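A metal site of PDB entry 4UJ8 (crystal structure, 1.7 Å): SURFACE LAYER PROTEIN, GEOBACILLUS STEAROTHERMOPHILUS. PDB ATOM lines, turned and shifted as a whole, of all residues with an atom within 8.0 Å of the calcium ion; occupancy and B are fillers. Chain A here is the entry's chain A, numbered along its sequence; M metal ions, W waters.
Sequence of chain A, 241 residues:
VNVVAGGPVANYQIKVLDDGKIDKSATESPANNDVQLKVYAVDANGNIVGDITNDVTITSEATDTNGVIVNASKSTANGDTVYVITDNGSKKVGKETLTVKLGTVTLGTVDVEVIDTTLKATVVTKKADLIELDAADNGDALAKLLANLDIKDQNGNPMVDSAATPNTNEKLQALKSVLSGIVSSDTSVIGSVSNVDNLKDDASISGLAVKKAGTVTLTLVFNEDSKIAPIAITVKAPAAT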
ATOM      1  N   VAL A  16      15.887  -2.741 -24.454  1.00  0.00           N
ATOM      2  CA  VAL A  16      14.801  -1.873 -24.916  1.00  0.00           C
ATOM      3  C   VAL A  16      15.035  -0.479 -24.355  1.00  0.00           C
ATOM      4  O   VAL A  16      15.093  -0.326 -23.140  1.00  0.00           O
ATOM      5  CB  VAL A  16      13.432  -2.419 -24.454  1.00  0.00           C
ATOM      6  CG1 VAL A  16      12.296  -1.459 -24.839  1.00  0.00           C
ATOM      7  CG2 VAL A  16      13.201  -3.833 -24.988  1.00  0.00           C
ATOM      8  N   LEU A  17      15.159   0.528 -25.226  1.00  0.00           N
ATOM      9  CA  LEU A  17      15.521   1.873 -24.781  1.00  0.00           C
ATOM     10  C   LEU A  17      14.288   2.666 -24.370  1.00  0.00           C
ATOM     11  O   LEU A  17      14.376   3.588 -23.563  1.00  0.00           O
ATOM     12  CB  LEU A  17      16.262   2.642 -25.877  1.00  0.00           C
ATOM     13  CG  LEU A  17      17.580   2.061 -26.413  1.00  0.00           C
ATOM     14  CD1 LEU A  17      18.161   2.950 -27.487  1.00  0.00           C
ATOM     15  CD2 LEU A  17      18.596   1.845 -25.285  1.00  0.00           C
ATOM     16  N   ASP A  18      13.153   2.314 -24.964  1.00  0.00           N
ATOM     17  CA  ASP A  18      11.899   3.018 -24.719  1.00  0.00           C
ATOM     18  C   ASP A  18      10.942   2.184 -23.861  1.00  0.00           C
ATOM     19  O   ASP A  18      11.370   1.516 -22.904  1.00  0.00           O
ATOM     20  CB  ASP A  18      11.240   3.389 -26.055  1.00  0.00           C
ATOM     21  CG  ASP A  18      10.838   2.168 -26.863  1.00  0.00           C
ATOM     22  OD1 ASP A  18      11.685   1.278 -27.071  1.00  0.00           O
ATOM     23  OD2 ASP A  18       9.656   2.102 -27.264  1.00  0.00           O
ATOM     24  N   ASP A  19       9.650   2.226 -24.170  1.00  0.00           N
ATOM     25  CA  ASP A  19       8.665   1.473 -23.396  1.00  0.00           C
ATOM     26  C   ASP A  19       8.327   0.100 -23.974  1.00  0.00           C
ATOM     27  O   ASP A  19       7.574  -0.664 -23.361  1.00  0.00           O
ATOM     28  CB  ASP A  19       7.391   2.299 -23.218  1.00  0.00           C
ATOM     29  CG  ASP A  19       6.608   2.486 -24.532  1.00  0.00           C
ATOM     30  OD1 ASP A  19       7.144   2.195 -25.618  1.00  0.00           O
ATOM     31  OD2 ASP A  19       5.453   2.937 -24.464  1.00  0.00           O
ATOM     32  N   GLY A  20       8.854  -0.206 -25.154  1.00  0.00           N
ATOM     33  CA  GLY A  20       8.616  -1.498 -25.769  1.00  0.00           C
ATOM     34  C   GLY A  20       7.259  -1.620 -26.425  1.00  0.00           C
ATOM     35  O   GLY A  20       6.859  -2.708 -26.847  1.00  0.00           O
ATOM     36  N   LYS A  21       6.553  -0.493 -26.533  1.00  0.00           N
ATOM     37  CA  LYS A  21       5.243  -0.471 -27.141  1.00  0.00           C
ATOM     38  C   LYS A  21       5.185   0.484 -28.337  1.00  0.00           C
ATOM     39  O   LYS A  21       5.940   1.447 -28.409  1.00  0.00           O
ATOM     40  CB  LYS A  21       4.192  -0.057 -26.118  1.00  0.00           C
ATOM     41  CG  LYS A  21       4.107  -0.951 -24.915  1.00  0.00           C
ATOM     42  CD  LYS A  21       3.179  -0.346 -23.861  1.00  0.00           C
ATOM     43  CE  LYS A  21       2.855  -1.345 -22.743  1.00  0.00           C
ATOM     44  NZ  LYS A  21       4.071  -2.047 -22.236  1.00  0.00           N
ATOM     45  N   ILE A  22       4.272   0.189 -29.255  1.00  0.00           N
ATOM     46  CA  ILE A  22       4.013   0.976 -30.451  1.00  0.00           C
ATOM     47  C   ILE A  22       2.524   1.316 -30.462  1.00  0.00           C
ATOM     48  O   ILE A  22       1.688   0.406 -30.458  1.00  0.00           O
ATOM     49  CB  ILE A  22       4.398   0.195 -31.729  1.00  0.00           C
ATOM     50  CG1 ILE A  22       5.879  -0.183 -31.692  1.00  0.00           C
ATOM     51  CG2 ILE A  22       4.006   0.953 -33.008  1.00  0.00           C
ATOM     52  CD1 ILE A  22       6.289  -1.136 -32.809  1.00  0.00           C
ATOM     53  N   ASP A  23       2.182   2.601 -30.449  1.00  0.00           N
ATOM     54  CA  ASP A  23       0.767   3.023 -30.315  1.00  0.00           C
ATOM     55  C   ASP A  23       0.233   3.440 -31.678  1.00  0.00           C
ATOM     56  O   ASP A  23       0.645   4.454 -32.242  1.00  0.00           O
ATOM     57  CB  ASP A  23       0.658   4.166 -29.286  1.00  0.00           C
ATOM     58  CG  ASP A  23      -0.778   4.518 -28.933  1.00  0.00           C
ATOM     59  OD1 ASP A  23      -1.696   4.127 -29.680  1.00  0.00           O
ATOM     60  OD2 ASP A  23      -0.989   5.208 -27.902  1.00  0.00           O
ATOM     61  N   GLU A  28      -1.676  10.010 -30.233  1.00  0.00           N
ATOM     62  CA  GLU A  28      -1.226   9.895 -28.852  1.00  0.00           C
ATOM     63  C   GLU A  28      -0.133  10.924 -28.534  1.00  0.00           C
ATOM     64  O   GLU A  28       0.692  11.260 -29.391  1.00  0.00           O
ATOM     65  CB  GLU A  28      -0.736   8.475 -28.504  1.00  0.00           C
ATOM     66  CG  GLU A  28       0.680   8.122 -28.978  1.00  0.00           C
ATOM     67  CD  GLU A  28       0.705   7.699 -30.433  1.00  0.00           C
ATOM     68  OE1 GLU A  28      -0.387   7.625 -31.049  1.00  0.00           O
ATOM     69  OE2 GLU A  28       1.806   7.432 -30.964  1.00  0.00           O
ATOM     70  N   ALA A  31       4.115  11.243 -28.823  1.00  0.00           N
ATOM     71  CA  ALA A  31       4.126  10.263 -29.907  1.00  0.00           C
ATOM     72  C   ALA A  31       4.855   9.020 -29.421  1.00  0.00           C
ATOM     73  O   ALA A  31       5.871   9.119 -28.734  1.00  0.00           O
ATOM     74  CB  ALA A  31       4.787  10.839 -31.135  1.00  0.00           C
ATOM     75  N   ASN A  32       4.313   7.861 -29.776  1.00  0.00           N
ATOM     76  CA  ASN A  32       4.822   6.580 -29.305  1.00  0.00           C
ATOM     77  C   ASN A  32       4.815   5.567 -30.443  1.00  0.00           C
ATOM     78  O   ASN A  32       4.073   4.584 -30.398  1.00  0.00           O
ATOM     79  CB  ASN A  32       3.985   6.086 -28.132  1.00  0.00           C
ATOM     80  CG  ASN A  32       4.598   4.886 -27.439  1.00  0.00           C
ATOM     81  OD1 ASN A  32       5.731   4.529 -27.734  1.00  0.00           O
ATOM     82  ND2 ASN A  32       3.862   4.263 -26.515  1.00  0.00           N
ATOM     83  N   ASN A  33       5.641   5.802 -31.463  1.00  0.00           N
ATOM     84  CA  ASN A  33       5.498   5.068 -32.712  1.00  0.00           C
ATOM     85  C   ASN A  33       6.627   4.105 -33.019  1.00  0.00           C
ATOM     86  O   ASN A  33       6.743   3.604 -34.143  1.00  0.00           O
ATOM     87  CB  ASN A  33       5.344   6.055 -33.863  1.00  0.00           C
ATOM     88  CG  ASN A  33       4.038   6.798 -33.777  1.00  0.00           C
ATOM     89  OD1 ASN A  33       2.996   6.192 -33.555  1.00  0.00           O
ATOM     90  ND2 ASN A  33       4.082   8.117 -33.926  1.00  0.00           N
ATOM     91  N   ASP A  34       7.464   3.831 -32.032  1.00  0.00           N
ATOM     92  CA  ASP A  34       8.463   2.815 -32.261  1.00  0.00           C
ATOM     93  C   ASP A  34       8.856   2.088 -30.997  1.00  0.00           C
ATOM     94  O   ASP A  34       8.384   2.411 -29.907  1.00  0.00           O
ATOM     95  CB  ASP A  34       9.731   3.410 -32.943  1.00  0.00           C
ATOM     96  CG  ASP A  34      10.459   4.444 -32.097  1.00  0.00           C
ATOM     97  OD1 ASP A  34      10.402   4.417 -30.850  1.00  0.00           O
ATOM     98  OD2 ASP A  34      11.146   5.299 -32.702  1.00  0.00           O
ATOM     99  N   VAL A  35       9.676   1.064 -31.203  1.00  0.00           N
ATOM    100  CA  VAL A  35      10.491   0.488 -30.151  1.00  0.00           C
ATOM    101  C   VAL A  35      11.927   0.633 -30.634  1.00  0.00           C
ATOM    102  O   VAL A  35      12.206   0.498 -31.829  1.00  0.00           O
ATOM    103  CB  VAL A  35      10.146  -1.002 -29.890  1.00  0.00           C
ATOM    104  CG1 VAL A  35      11.119  -1.630 -28.878  1.00  0.00           C
ATOM    105  CG2 VAL A  35       8.718  -1.123 -29.384  1.00  0.00           C
ATOM    106  N   GLN A  36      12.815   0.962 -29.716  1.00  0.00           N
ATOM    107  CA  GLN A  36      14.222   1.162 -30.039  1.00  0.00           C
ATOM    108  C   GLN A  36      15.086   0.169 -29.276  1.00  0.00           C
ATOM    109  O   GLN A  36      14.986   0.079 -28.052  1.00  0.00           O
ATOM    110  CB  GLN A  36      14.623   2.596 -29.711  1.00  0.00           C
ATOM    111  CG  GLN A  36      13.710   3.634 -30.363  1.00  0.00           C
ATOM    112  CD  GLN A  36      13.621   4.900 -29.555  1.00  0.00           C
ATOM    113  OE1 GLN A  36      14.626   5.343 -28.981  1.00  0.00           O
ATOM    114  NE2 GLN A  36      12.426   5.477 -29.457  1.00  0.00           N
ATOM    115  N   ILE A  85      11.986  -0.428 -34.451  1.00  0.00           N
ATOM    116  CA  ILE A  85      10.841  -1.264 -34.736  1.00  0.00           C
ATOM    117  C   ILE A  85       9.627  -0.380 -34.891  1.00  0.00           C
ATOM    118  O   ILE A  85       9.345   0.458 -34.047  1.00  0.00           O
ATOM    119  CB  ILE A  85      10.612  -2.293 -33.631  1.00  0.00           C
ATOM    120  CG1 ILE A  85      11.957  -2.924 -33.219  1.00  0.00           C
ATOM    121  CG2 ILE A  85       9.561  -3.321 -34.060  1.00  0.00           C
ATOM    122  CD1 ILE A  85      12.697  -3.636 -34.357  1.00  0.00           C
ATOM    123  N   GLU A 113       5.069  -4.746 -28.385  1.00  0.00           N
ATOM    124  CA  GLU A 113       3.611  -4.763 -28.320  1.00  0.00           C
ATOM    125  C   GLU A 113       3.021  -3.602 -29.076  1.00  0.00           C
ATOM    126  O   GLU A 113       3.440  -2.442 -28.882  1.00  0.00           O
ATOM    127  CB  GLU A 113       3.130  -4.735 -26.877  1.00  0.00           C
ATOM    128  CG  GLU A 113       1.662  -5.105 -26.716  1.00  0.00           C
ATOM    129  CD  GLU A 113       1.147  -4.831 -25.327  1.00  0.00           C
ATOM    130  OE1 GLU A 113       1.970  -4.454 -24.470  1.00  0.00           O
ATOM    131  OE2 GLU A 113      -0.081  -4.979 -25.092  1.00  0.00           O
ATOM    132  N   ILE A 115      -0.168  -1.303 -29.413  1.00  0.00           N
ATOM    133  CA  ILE A 115      -1.345  -0.894 -28.656  1.00  0.00           C
ATOM    134  C   ILE A 115      -2.101   0.152 -29.461  1.00  0.00           C
ATOM    135  O   ILE A 115      -1.662   0.571 -30.528  1.00  0.00           O
ATOM    136  CB  ILE A 115      -0.994  -0.313 -27.257  1.00  0.00           C
ATOM    137  CG1 ILE A 115      -0.224   0.998 -27.395  1.00  0.00           C
ATOM    138  CG2 ILE A 115      -0.185  -1.327 -26.436  1.00  0.00           C
ATOM    139  CD1 ILE A 115       0.064   1.695 -26.067  1.00  0.00           C
HETATM  140 CA    CA M   1       7.601   3.123 -27.737  1.00  0.00          CA
HETATM  141  O   HOH W   1       7.956   4.983 -26.053  1.00  0.00           O
HETATM  142  O   HOH W   2       8.494   5.081 -28.974  1.00  0.00           O
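The backbone carbonyl oxygen (O) of Asn 32 is in hydrogen-bond range of the backbone NH (N) of Asp 23 (2.7 Å). OD2 of Asp 18 sits close to N of Gly 20 (3.2 Å). The side-chain carboxylate of Glu 113 lies within salt-bridge range of the side-chain amino group of Lys 21 (3.9 Å). NE2 of Gln 36 sits at hydrogen-bond distance from OD1 of Asp 34, 2.7 Å away. The side-chain carboxylate (OD1) of Asp 18 lies within hydrogen-bond range of the backbone NH (N) of Gln 36 (2.9 Å). The side-chain carboxylate (OE2) of Glu 28 sits close to the backbone NH (N) of Asn 32 (2.8 Å).
Of the 18 residues printed, 5 come within 4 Å of the calcium ion. The nearest printed residue that does not touch the calcium ion is Gly 20 (4.4 Å).
The calcium ion is bound by the side-chain amide oxygen (OD1) of Asn 32, 2.3 Å away. The side-chain carboxylate (OD2) of Asp 18 binds the calcium ion (2.3 Å). The calcium ion is bound by the side-chain carboxylate (OD1) of Asp 19 (2.4 Å). O of Asp 34 binds the calcium ion. O of Lys 21 is bound to the calcium ion. The calcium ion is bound by water W2 (2.5 Å). The calcium ion is bound by water W1 (2.5 Å).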
